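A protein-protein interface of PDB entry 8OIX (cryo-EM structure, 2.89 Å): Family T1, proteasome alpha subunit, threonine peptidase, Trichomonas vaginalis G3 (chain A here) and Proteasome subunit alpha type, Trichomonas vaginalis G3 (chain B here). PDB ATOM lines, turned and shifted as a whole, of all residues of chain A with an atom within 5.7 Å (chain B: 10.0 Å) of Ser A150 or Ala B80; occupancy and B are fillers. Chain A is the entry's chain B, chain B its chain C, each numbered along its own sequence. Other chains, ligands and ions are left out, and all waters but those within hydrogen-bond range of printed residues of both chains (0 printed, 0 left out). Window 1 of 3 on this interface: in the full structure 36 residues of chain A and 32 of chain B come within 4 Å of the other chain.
Among the printed residues, no Asp or Glu carboxylate lies within 4 Å of a Lys or Arg side-chain nitrogen of the other chain.
The indole nitrogen (NE1) of Trp A154 lies close to the side-chain amide nitrogen (ND2) of Asn B51 (3.2 Å). The side-chain amide oxygen of Gln A117 is in hydrogen-bond range of the side-chain hydroxyl of Thr B84, 2.7 Å away. The side-chain carboxylate (OD1) of Asp B81 lies close to the side-chain amide nitrogen (NE2) of Gln A117, at 2.4 Å. The backbone carbonyl oxygen (O) of Thr A120 lies within hydrogen-bond range of the guanidinium group (NE) of Arg B127 (3.2 Å). The guanidinium group of Arg B127 sits close to the side-chain amide nitrogen of Gln A117.
The side-chain hydroxyl (OG1) of Thr A120 lies within hydrogen-bond range of the backbone carbonyl oxygen (O) of Gln A117, 2.6 Å away. OG1 of Thr A152 lies within hydrogen-bond range of OG of Ser A150 (2.7 Å). The side-chain carboxylate (OD1) of Asp B81 is in salt-bridge range of the guanidinium group (NH2) of Arg B127, at 2.9 Å. The backbone NH (N) of Lys B50 lies within hydrogen-bond range of the side-chain carboxylate (OE1) of Glu B62. The backbone NH of Gly B130 lies within hydrogen-bond range of the side-chain carboxylate of Asp B81 (3.3 Å). N of Asn B51 is in hydrogen-bond range of OE1 of Glu B62, 3.3 Å away.
Among the printed residues, merely in contact across the chains: Gln A117 with Ala B80, Ser A150 with Ala B80, Gly A151 with Ala B80, Thr A152 with Thr B79, Thr A152 with Ala B80 and Trp A154 with Lys B50.
Ser A150 touches just one residue of chain B: Ala B80. No residue of chain B comes within 4 Å of Asp A148. Of chain B, only Ala B80 comes within 4 Å of Gly A151. Of the printed residues of chain A, Lys B50 touches Trp A154 (3.3 Å). Printed residues of chain A within 4 Å of Asn B51: Trp A154 (2.9 Å). Val B75 touches none of the printed residues of chain A. The nearest residue of chain A that does not touch Ala B80 is Ala A113 (5.0 Å).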
ATOM      1  N   ILE A  20     -24.250   6.524   8.445  1.00  0.00           N
ATOM      2  CA  ILE A  20     -25.470   5.885   7.958  1.00  0.00           C
ATOM      3  C   ILE A  20     -25.659   4.525   8.611  1.00  0.00           C
ATOM      4  O   ILE A  20     -26.765   4.173   9.032  1.00  0.00           O
ATOM      5  CB  ILE A  20     -25.447   5.777   6.423  1.00  0.00           C
ATOM      6  CG1 ILE A  20     -25.418   7.171   5.813  1.00  0.00           C
ATOM      7  CG2 ILE A  20     -26.650   4.996   5.930  1.00  0.00           C
ATOM      8  CD1 ILE A  20     -26.594   7.984   6.194  1.00  0.00           C
ATOM      9  N   LEU A  24     -28.653   3.391  11.044  1.00  0.00           N
ATOM     10  CA  LEU A  24     -29.382   2.154  10.784  1.00  0.00           C
ATOM     11  C   LEU A  24     -29.369   1.239  12.002  1.00  0.00           C
ATOM     12  O   LEU A  24     -30.358   0.554  12.283  1.00  0.00           O
ATOM     13  CB  LEU A  24     -28.791   1.446   9.567  1.00  0.00           C
ATOM     14  CG  LEU A  24     -29.128   2.064   8.210  1.00  0.00           C
ATOM     15  CD1 LEU A  24     -28.137   1.610   7.153  1.00  0.00           C
ATOM     16  CD2 LEU A  24     -30.544   1.701   7.804  1.00  0.00           C
ATOM     17  N   ALA A 113     -37.403  11.120   2.246  1.00  0.00           N
ATOM     18  CA  ALA A 113     -36.096  10.666   1.795  1.00  0.00           C
ATOM     19  C   ALA A 113     -35.173  11.839   1.499  1.00  0.00           C
ATOM     20  O   ALA A 113     -33.983  11.797   1.825  1.00  0.00           O
ATOM     21  CB  ALA A 113     -36.264   9.789   0.558  1.00  0.00           C
ATOM     22  N   MET A 116     -34.019  13.337   4.823  1.00  0.00           N
ATOM     23  CA  MET A 116     -33.045  12.483   5.485  1.00  0.00           C
ATOM     24  C   MET A 116     -31.700  12.514   4.769  1.00  0.00           C
ATOM     25  O   MET A 116     -30.656  12.614   5.416  1.00  0.00           O
ATOM     26  CB  MET A 116     -33.592  11.064   5.596  1.00  0.00           C
ATOM     27  CG  MET A 116     -34.851  11.015   6.437  1.00  0.00           C
ATOM     28  SD  MET A 116     -35.692   9.432   6.419  1.00  0.00           S
ATOM     29  CE  MET A 116     -35.030   8.738   7.918  1.00  0.00           C
ATOM     30  N   GLN A 117     -31.703  12.466   3.435  1.00  0.00           N
ATOM     31  CA  GLN A 117     -30.456  12.589   2.686  1.00  0.00           C
ATOM     32  C   GLN A 117     -29.786  13.929   2.956  1.00  0.00           C
ATOM     33  O   GLN A 117     -28.562  14.000   3.139  1.00  0.00           O
ATOM     34  CB  GLN A 117     -30.732  12.412   1.191  1.00  0.00           C
ATOM     35  CG  GLN A 117     -29.496  12.266   0.313  1.00  0.00           C
ATOM     36  CD  GLN A 117     -28.793  13.579   0.041  1.00  0.00           C
ATOM     37  OE1 GLN A 117     -29.430  14.626  -0.066  1.00  0.00           O
ATOM     38  NE2 GLN A 117     -27.473  13.529  -0.075  1.00  0.00           N
ATOM     39  N   THR A 120     -28.040  13.712   5.968  1.00  0.00           N
ATOM     40  CA  THR A 120     -26.850  12.880   5.830  1.00  0.00           C
ATOM     41  C   THR A 120     -25.732  13.571   5.065  1.00  0.00           C
ATOM     42  O   THR A 120     -24.609  13.057   5.046  1.00  0.00           O
ATOM     43  CB  THR A 120     -27.163  11.555   5.133  1.00  0.00           C
ATOM     44  OG1 THR A 120     -27.417  11.785   3.742  1.00  0.00           O
ATOM     45  CG2 THR A 120     -28.345  10.883   5.771  1.00  0.00           C
ATOM     46  N   PRO A 127     -27.419  11.883  10.682  1.00  0.00           N
ATOM     47  CA  PRO A 127     -28.604  11.378   9.986  1.00  0.00           C
ATOM     48  C   PRO A 127     -29.708  11.049  10.977  1.00  0.00           C
ATOM     49  O   PRO A 127     -29.452  10.700  12.130  1.00  0.00           O
ATOM     50  CB  PRO A 127     -28.097  10.119   9.273  1.00  0.00           C
ATOM     51  CG  PRO A 127     -26.618  10.237   9.267  1.00  0.00           C
ATOM     52  CD  PRO A 127     -26.256  11.002  10.494  1.00  0.00           C
ATOM     53  N   ASP A 148     -35.097   4.870   4.781  1.00  0.00           N
ATOM     54  CA  ASP A 148     -33.994   4.623   5.696  1.00  0.00           C
ATOM     55  C   ASP A 148     -33.335   5.931   6.101  1.00  0.00           C
ATOM     56  O   ASP A 148     -33.580   6.982   5.505  1.00  0.00           O
ATOM     57  CB  ASP A 148     -32.996   3.663   5.054  1.00  0.00           C
ATOM     58  CG  ASP A 148     -33.314   2.215   5.364  1.00  0.00           C
ATOM     59  OD1 ASP A 148     -33.861   1.953   6.456  1.00  0.00           O
ATOM     60  OD2 ASP A 148     -33.011   1.339   4.534  1.00  0.00           O
ATOM     61  N   PRO A 149     -32.500   5.905   7.145  1.00  0.00           N
ATOM     62  CA  PRO A 149     -31.747   7.116   7.505  1.00  0.00           C
ATOM     63  C   PRO A 149     -30.915   7.680   6.374  1.00  0.00           C
ATOM     64  O   PRO A 149     -30.730   8.900   6.308  1.00  0.00           O
ATOM     65  CB  PRO A 149     -30.861   6.634   8.659  1.00  0.00           C
ATOM     66  CG  PRO A 149     -31.629   5.531   9.267  1.00  0.00           C
ATOM     67  CD  PRO A 149     -32.300   4.830   8.131  1.00  0.00           C
ATOM     68  N   SER A 150     -30.409   6.832   5.477  1.00  0.00           N
ATOM     69  CA  SER A 150     -29.642   7.326   4.342  1.00  0.00           C
ATOM     70  C   SER A 150     -30.478   8.196   3.418  1.00  0.00           C
ATOM     71  O   SER A 150     -29.912   8.962   2.631  1.00  0.00           O
ATOM     72  CB  SER A 150     -29.062   6.154   3.550  1.00  0.00           C
ATOM     73  OG  SER A 150     -30.040   5.153   3.334  1.00  0.00           O
ATOM     74  N   GLY A 151     -31.799   8.126   3.522  1.00  0.00           N
ATOM     75  CA  GLY A 151     -32.682   8.728   2.548  1.00  0.00           C
ATOM     76  C   GLY A 151     -32.997   7.852   1.360  1.00  0.00           C
ATOM     77  O   GLY A 151     -33.632   8.327   0.412  1.00  0.00           O
ATOM     78  N   THR A 152     -32.536   6.608   1.354  1.00  0.00           N
ATOM     79  CA  THR A 152     -32.933   5.650   0.334  1.00  0.00           C
ATOM     80  C   THR A 152     -34.262   5.022   0.733  1.00  0.00           C
ATOM     81  O   THR A 152     -34.430   4.589   1.877  1.00  0.00           O
ATOM     82  CB  THR A 152     -31.853   4.585   0.162  1.00  0.00           C
ATOM     83  OG1 THR A 152     -31.556   3.998   1.433  1.00  0.00           O
ATOM     84  CG2 THR A 152     -30.588   5.202  -0.395  1.00  0.00           C
ATOM     85  N   TRP A 154     -37.034   2.122  -0.086  1.00  0.00           N
ATOM     86  CA  TRP A 154     -37.573   0.916  -0.681  1.00  0.00           C
ATOM     87  C   TRP A 154     -39.082   1.054  -0.830  1.00  0.00           C
ATOM     88  O   TRP A 154     -39.730   1.837  -0.131  1.00  0.00           O
ATOM     89  CB  TRP A 154     -37.367  -0.324   0.201  1.00  0.00           C
ATOM     90  CG  TRP A 154     -36.000  -0.850   0.564  1.00  0.00           C
ATOM     91  CD1 TRP A 154     -35.673  -2.167   0.705  1.00  0.00           C
ATOM     92  CD2 TRP A 154     -34.834  -0.112   0.968  1.00  0.00           C
ATOM     93  NE1 TRP A 154     -34.369  -2.301   1.097  1.00  0.00           N
ATOM     94  CE2 TRP A 154     -33.831  -1.055   1.277  1.00  0.00           C
ATOM     95  CE3 TRP A 154     -34.529   1.246   1.069  1.00  0.00           C
ATOM     96  CZ2 TRP A 154     -32.550  -0.681   1.665  1.00  0.00           C
ATOM     97  CZ3 TRP A 154     -33.263   1.610   1.458  1.00  0.00           C
ATOM     98  CH2 TRP A 154     -32.286   0.654   1.749  1.00  0.00           C
ATOM     99  N   SER B  27     -17.854   3.159  -3.159  1.00  0.00           N
ATOM    100  CA  SER B  27     -19.251   2.908  -2.819  1.00  0.00           C
ATOM    101  C   SER B  27     -20.070   2.618  -4.068  1.00  0.00           C
ATOM    102  O   SER B  27     -20.937   1.737  -4.063  1.00  0.00           O
ATOM    103  CB  SER B  27     -19.828   4.106  -2.067  1.00  0.00           C
ATOM    104  OG  SER B  27     -21.218   3.951  -1.848  1.00  0.00           O
ATOM    105  N   ALA B  31     -22.253  -0.847  -5.609  1.00  0.00           N
ATOM    106  CA  ALA B  31     -23.667  -0.703  -5.918  1.00  0.00           C
ATOM    107  C   ALA B  31     -24.051  -1.526  -7.144  1.00  0.00           C
ATOM    108  O   ALA B  31     -23.203  -2.029  -7.883  1.00  0.00           O
ATOM    109  CB  ALA B  31     -24.020   0.768  -6.133  1.00  0.00           C
ATOM    110  N   LYS B  50     -31.273  -1.878  -6.098  1.00  0.00           N
ATOM    111  CA  LYS B  50     -30.607  -2.128  -4.827  1.00  0.00           C
ATOM    112  C   LYS B  50     -31.505  -2.897  -3.873  1.00  0.00           C
ATOM    113  O   LYS B  50     -31.011  -3.680  -3.053  1.00  0.00           O
ATOM    114  CB  LYS B  50     -30.174  -0.806  -4.192  1.00  0.00           C
ATOM    115  CG  LYS B  50     -29.389  -0.947  -2.902  1.00  0.00           C
ATOM    116  CD  LYS B  50     -29.020   0.417  -2.341  1.00  0.00           C
ATOM    117  CE  LYS B  50     -28.490   0.307  -0.923  1.00  0.00           C
ATOM    118  NZ  LYS B  50     -29.552  -0.131   0.024  1.00  0.00           N
ATOM    119  N   ASN B  51     -32.814  -2.700  -3.972  1.00  0.00           N
ATOM    120  CA  ASN B  51     -33.784  -3.319  -3.077  1.00  0.00           C
ATOM    121  C   ASN B  51     -34.478  -4.422  -3.868  1.00  0.00           C
ATOM    122  O   ASN B  51     -35.390  -4.151  -4.654  1.00  0.00           O
ATOM    123  CB  ASN B  51     -34.773  -2.275  -2.578  1.00  0.00           C
ATOM    124  CG  ASN B  51     -34.097  -0.964  -2.235  1.00  0.00           C
ATOM    125  OD1 ASN B  51     -34.497   0.096  -2.714  1.00  0.00           O
ATOM    126  ND2 ASN B  51     -33.015  -1.039  -1.475  1.00  0.00           N
ATOM    127  N   GLU B  62     -36.141   2.609  -9.227  1.00  0.00           N
ATOM    128  CA  GLU B  62     -35.251   3.032  -8.155  1.00  0.00           C
ATOM    129  C   GLU B  62     -33.958   3.634  -8.687  1.00  0.00           C
ATOM    130  O   GLU B  62     -33.584   4.746  -8.302  1.00  0.00           O
ATOM    131  CB  GLU B  62     -34.933   1.844  -7.240  1.00  0.00           C
ATOM    132  CG  GLU B  62     -34.089   2.209  -6.043  1.00  0.00           C
ATOM    133  CD  GLU B  62     -33.053   1.157  -5.727  1.00  0.00           C
ATOM    134  OE1 GLU B  62     -33.348  -0.044  -5.905  1.00  0.00           O
ATOM    135  OE2 GLU B  62     -31.941   1.534  -5.305  1.00  0.00           O
ATOM    136  N   LYS B  63     -33.267   2.915  -9.569  1.00  0.00           N
ATOM    137  CA  LYS B  63     -32.021   3.395 -10.149  1.00  0.00           C
ATOM    138  C   LYS B  63     -32.238   4.256 -11.384  1.00  0.00           C
ATOM    139  O   LYS B  63     -31.304   4.937 -11.820  1.00  0.00           O
ATOM    140  CB  LYS B  63     -31.122   2.212 -10.512  1.00  0.00           C
ATOM    141  CG  LYS B  63     -30.787   1.291  -9.353  1.00  0.00           C
ATOM    142  CD  LYS B  63     -29.773   1.915  -8.417  1.00  0.00           C
ATOM    143  CE  LYS B  63     -29.309   0.914  -7.373  1.00  0.00           C
ATOM    144  NZ  LYS B  63     -28.116   1.401  -6.630  1.00  0.00           N
ATOM    145  N   VAL B  75     -28.390   5.324 -12.358  1.00  0.00           N
ATOM    146  CA  VAL B  75     -27.478   5.721 -11.294  1.00  0.00           C
ATOM    147  C   VAL B  75     -26.899   4.491 -10.612  1.00  0.00           C
ATOM    148  O   VAL B  75     -27.601   3.500 -10.385  1.00  0.00           O
ATOM    149  CB  VAL B  75     -28.154   6.648 -10.264  1.00  0.00           C
ATOM    150  CG1 VAL B  75     -29.239   5.910  -9.494  1.00  0.00           C
ATOM    151  CG2 VAL B  75     -27.102   7.218  -9.332  1.00  0.00           C
ATOM    152  N   ALA B  76     -25.601   4.544 -10.323  1.00  0.00           N
ATOM    153  CA  ALA B  76     -24.952   3.582  -9.446  1.00  0.00           C
ATOM    154  C   ALA B  76     -24.438   4.315  -8.217  1.00  0.00           C
ATOM    155  O   ALA B  76     -23.821   5.378  -8.337  1.00  0.00           O
ATOM    156  CB  ALA B  76     -23.809   2.856 -10.156  1.00  0.00           C
ATOM    157  N   GLY B  77     -24.691   3.752  -7.041  1.00  0.00           N
ATOM    158  CA  GLY B  77     -24.266   4.381  -5.807  1.00  0.00           C
ATOM    159  C   GLY B  77     -25.411   4.676  -4.864  1.00  0.00           C
ATOM    160  O   GLY B  77     -26.452   4.014  -4.916  1.00  0.00           O
ATOM    161  N   LEU B  78     -25.225   5.663  -3.991  1.00  0.00           N
ATOM    162  CA  LEU B  78     -26.243   6.005  -3.007  1.00  0.00           C
ATOM    163  C   LEU B  78     -27.514   6.477  -3.698  1.00  0.00           C
ATOM    164  O   LEU B  78     -27.522   7.517  -4.359  1.00  0.00           O
ATOM    165  CB  LEU B  78     -25.716   7.085  -2.065  1.00  0.00           C
ATOM    166  CG  LEU B  78     -24.426   6.736  -1.323  1.00  0.00           C
ATOM    167  CD1 LEU B  78     -24.013   7.879  -0.415  1.00  0.00           C
ATOM    168  CD2 LEU B  78     -24.602   5.452  -0.533  1.00  0.00           C
ATOM    169  N   THR B  79     -28.595   5.714  -3.538  1.00  0.00           N
ATOM    170  CA  THR B  79     -29.838   6.061  -4.217  1.00  0.00           C
ATOM    171  C   THR B  79     -30.415   7.373  -3.700  1.00  0.00           C
ATOM    172  O   THR B  79     -31.118   8.068  -4.437  1.00  0.00           O
ATOM    173  CB  THR B  79     -30.857   4.934  -4.060  1.00  0.00           C
ATOM    174  OG1 THR B  79     -30.190   3.671  -4.168  1.00  0.00           O
ATOM    175  CG2 THR B  79     -31.917   5.027  -5.143  1.00  0.00           C
ATOM    176  N   ALA B  80     -30.139   7.724  -2.444  1.00  0.00           N
ATOM    177  CA  ALA B  80     -30.646   8.975  -1.891  1.00  0.00           C
ATOM    178  C   ALA B  80     -29.967  10.184  -2.524  1.00  0.00           C
ATOM    179  O   ALA B  80     -30.632  11.148  -2.927  1.00  0.00           O
ATOM    180  CB  ALA B  80     -30.452   8.984  -0.382  1.00  0.00           C
ATOM    181  N   ASP B  81     -28.633  10.159  -2.596  1.00  0.00           N
ATOM    182  CA  ASP B  81     -27.915  11.204  -3.317  1.00  0.00           C
ATOM    183  C   ASP B  81     -28.355  11.240  -4.771  1.00  0.00           C
ATOM    184  O   ASP B  81     -28.420  12.310  -5.387  1.00  0.00           O
ATOM    185  CB  ASP B  81     -26.407  10.973  -3.218  1.00  0.00           C
ATOM    186  CG  ASP B  81     -25.880  11.153  -1.812  1.00  0.00           C
ATOM    187  OD1 ASP B  81     -26.686  11.432  -0.903  1.00  0.00           O
ATOM    188  OD2 ASP B  81     -24.654  11.014  -1.615  1.00  0.00           O
ATOM    189  N   ALA B  82     -28.665  10.071  -5.333  1.00  0.00           N
ATOM    190  CA  ALA B  82     -29.171  10.009  -6.696  1.00  0.00           C
ATOM    191  C   ALA B  82     -30.500  10.733  -6.825  1.00  0.00           C
ATOM    192  O   ALA B  82     -30.715  11.473  -7.785  1.00  0.00           O
ATOM    193  CB  ALA B  82     -29.327   8.554  -7.123  1.00  0.00           C
ATOM    194  N   ASN B  83     -31.404  10.534  -5.866  1.00  0.00           N
ATOM    195  CA  ASN B  83     -32.687  11.228  -5.901  1.00  0.00           C
ATOM    196  C   ASN B  83     -32.500  12.730  -5.761  1.00  0.00           C
ATOM    197  O   ASN B  83     -33.163  13.514  -6.449  1.00  0.00           O
ATOM    198  CB  ASN B  83     -33.599  10.693  -4.798  1.00  0.00           C
ATOM    199  CG  ASN B  83     -33.821   9.202  -4.901  1.00  0.00           C
ATOM    200  OD1 ASN B  83     -33.887   8.648  -5.997  1.00  0.00           O
ATOM    201  ND2 ASN B  83     -33.918   8.539  -3.757  1.00  0.00           N
ATOM    202  N   THR B  84     -31.600  13.148  -4.870  1.00  0.00           N
ATOM    203  CA  THR B  84     -31.340  14.575  -4.695  1.00  0.00           C
ATOM    204  C   THR B  84     -30.810  15.197  -5.981  1.00  0.00           C
ATOM    205  O   THR B  84     -31.301  16.240  -6.435  1.00  0.00           O
ATOM    206  CB  THR B  84     -30.353  14.789  -3.547  1.00  0.00           C
ATOM    207  OG1 THR B  84     -30.959  14.388  -2.313  1.00  0.00           O
ATOM    208  CG2 THR B  84     -29.950  16.252  -3.456  1.00  0.00           C
ATOM    209  N   LEU B  85     -29.813  14.559  -6.596  1.00  0.00           N
ATOM    210  CA  LEU B  85     -29.250  15.101  -7.825  1.00  0.00           C
ATOM    211  C   LEU B  85     -30.209  14.974  -8.998  1.00  0.00           C
ATOM    212  O   LEU B  85     -30.137  15.773  -9.931  1.00  0.00           O
ATOM    213  CB  LEU B  85     -27.926  14.422  -8.148  1.00  0.00           C
ATOM    214  CG  LEU B  85     -26.784  14.852  -7.238  1.00  0.00           C
ATOM    215  CD1 LEU B  85     -25.537  14.127  -7.638  1.00  0.00           C
ATOM    216  CD2 LEU B  85     -26.581  16.354  -7.314  1.00  0.00           C
ATOM    217  N   VAL B  86     -31.115  14.000  -8.972  1.00  0.00           N
ATOM    218  CA  VAL B  86     -32.128  13.911 -10.016  1.00  0.00           C
ATOM    219  C   VAL B  86     -33.126  15.049  -9.882  1.00  0.00           C
ATOM    220  O   VAL B  86     -33.550  15.637 -10.881  1.00  0.00           O
ATOM    221  CB  VAL B  86     -32.815  12.534  -9.981  1.00  0.00           C
ATOM    222  CG1 VAL B  86     -34.159  12.593 -10.677  1.00  0.00           C
ATOM    223  CG2 VAL B  86     -31.930  11.497 -10.648  1.00  0.00           C
ATOM    224  N   ASP B  87     -33.513  15.383  -8.652  1.00  0.00           N
ATOM    225  CA  ASP B  87     -34.358  16.553  -8.446  1.00  0.00           C
ATOM    226  C   ASP B  87     -33.655  17.818  -8.920  1.00  0.00           C
ATOM    227  O   ASP B  87     -34.260  18.666  -9.589  1.00  0.00           O
ATOM    228  CB  ASP B  87     -34.745  16.669  -6.973  1.00  0.00           C
ATOM    229  CG  ASP B  87     -35.905  17.619  -6.746  1.00  0.00           C
ATOM    230  OD1 ASP B  87     -36.532  18.045  -7.740  1.00  0.00           O
ATOM    231  OD2 ASP B  87     -36.192  17.939  -5.574  1.00  0.00           O
ATOM    232  N   LEU B  88     -32.364  17.950  -8.600  1.00  0.00           N
ATOM    233  CA  LEU B  88     -31.604  19.114  -9.052  1.00  0.00           C
ATOM    234  C   LEU B  88     -31.498  19.158 -10.573  1.00  0.00           C
ATOM    235  O   LEU B  88     -31.622  20.228 -11.178  1.00  0.00           O
ATOM    236  CB  LEU B  88     -30.215  19.117  -8.416  1.00  0.00           C
ATOM    237  CG  LEU B  88     -30.037  19.889  -7.105  1.00  0.00           C
ATOM    238  CD1 LEU B  88     -31.089  19.506  -6.075  1.00  0.00           C
ATOM    239  CD2 LEU B  88     -28.642  19.672  -6.548  1.00  0.00           C
ATOM    240  N   ARG B 127     -20.122  16.161   2.441  1.00  0.00           N
ATOM    241  CA  ARG B 127     -19.896  14.851   1.857  1.00  0.00           C
ATOM    242  C   ARG B 127     -20.136  14.904   0.351  1.00  0.00           C
ATOM    243  O   ARG B 127     -21.091  15.542  -0.104  1.00  0.00           O
ATOM    244  CB  ARG B 127     -20.827  13.828   2.502  1.00  0.00           C
ATOM    245  CG  ARG B 127     -20.730  12.440   1.923  1.00  0.00           C
ATOM    246  CD  ARG B 127     -21.721  11.507   2.582  1.00  0.00           C
ATOM    247  NE  ARG B 127     -23.096  11.973   2.450  1.00  0.00           N
ATOM    248  CZ  ARG B 127     -23.861  11.750   1.391  1.00  0.00           C
ATOM    249  NH1 ARG B 127     -23.404  11.102   0.333  1.00  0.00           N
ATOM    250  NH2 ARG B 127     -25.115  12.191   1.392  1.00  0.00           N
ATOM    251  N   PRO B 128     -19.293  14.255  -0.447  1.00  0.00           N
ATOM    252  CA  PRO B 128     -19.533  14.216  -1.890  1.00  0.00           C
ATOM    253  C   PRO B 128     -20.770  13.396  -2.215  1.00  0.00           C
ATOM    254  O   PRO B 128     -21.223  12.560  -1.433  1.00  0.00           O
ATOM    255  CB  PRO B 128     -18.265  13.553  -2.443  1.00  0.00           C
ATOM    256  CG  PRO B 128     -17.243  13.754  -1.369  1.00  0.00           C
ATOM    257  CD  PRO B 128     -18.020  13.605  -0.101  1.00  0.00           C
ATOM    258  N   TYR B 129     -21.317  13.650  -3.399  1.00  0.00           N
ATOM    259  CA  TYR B 129     -22.438  12.863  -3.902  1.00  0.00           C
ATOM    260  C   TYR B 129     -21.902  11.523  -4.385  1.00  0.00           C
ATOM    261  O   TYR B 129     -21.308  11.429  -5.460  1.00  0.00           O
ATOM    262  CB  TYR B 129     -23.161  13.602  -5.019  1.00  0.00           C
ATOM    263  CG  TYR B 129     -24.087  14.696  -4.545  1.00  0.00           C
ATOM    264  CD1 TYR B 129     -25.295  14.390  -3.936  1.00  0.00           C
ATOM    265  CD2 TYR B 129     -23.763  16.033  -4.722  1.00  0.00           C
ATOM    266  CE1 TYR B 129     -26.151  15.382  -3.509  1.00  0.00           C
ATOM    267  CE2 TYR B 129     -24.613  17.032  -4.297  1.00  0.00           C
ATOM    268  CZ  TYR B 129     -25.804  16.702  -3.689  1.00  0.00           C
ATOM    269  OH  TYR B 129     -26.656  17.694  -3.263  1.00  0.00           O
ATOM    270  N   GLY B 130     -22.115  10.481  -3.590  1.00  0.00           N
ATOM    271  CA  GLY B 130     -21.607   9.165  -3.921  1.00  0.00           C
ATOM    272  C   GLY B 130     -22.433   8.481  -4.988  1.00  0.00           C
ATOM    273  O   GLY B 130     -22.971   7.394  -4.762  1.00  0.00           O
ATOM    274  N   VAL B 131     -22.543   9.108  -6.157  1.00  0.00           N
ATOM    275  CA  VAL B 131     -23.363   8.595  -7.247  1.00  0.00           C
ATOM    276  C   VAL B 131     -22.626   8.791  -8.560  1.00  0.00           C
ATOM    277  O   VAL B 131     -21.924   9.788  -8.755  1.00  0.00           O
ATOM    278  CB  VAL B 131     -24.746   9.277  -7.313  1.00  0.00           C
ATOM    279  CG1 VAL B 131     -25.522   9.034  -6.052  1.00  0.00           C
ATOM    280  CG2 VAL B 131     -24.598  10.760  -7.560  1.00  0.00           C
ATOM    281  N   PHE B 133     -23.783   8.845 -12.512  1.00  0.00           N
ATOM    282  CA  PHE B 133     -24.921   8.867 -13.415  1.00  0.00           C
ATOM    283  C   PHE B 133     -24.518   8.438 -14.818  1.00  0.00           C
ATOM    284  O   PHE B 133     -23.510   8.898 -15.360  1.00  0.00           O
ATOM    285  CB  PHE B 133     -25.546  10.261 -13.466  1.00  0.00           C
ATOM    286  CG  PHE B 133     -26.371  10.605 -12.265  1.00  0.00           C
ATOM    287  CD1 PHE B 133     -27.555   9.936 -12.010  1.00  0.00           C
ATOM    288  CD2 PHE B 133     -25.973  11.605 -11.397  1.00  0.00           C
ATOM    289  CE1 PHE B 133     -28.321  10.253 -10.909  1.00  0.00           C
ATOM    290  CE2 PHE B 133     -26.735  11.926 -10.294  1.00  0.00           C
ATOM    291  CZ  PHE B 133     -27.911  11.249 -10.050  1.00  0.00           C
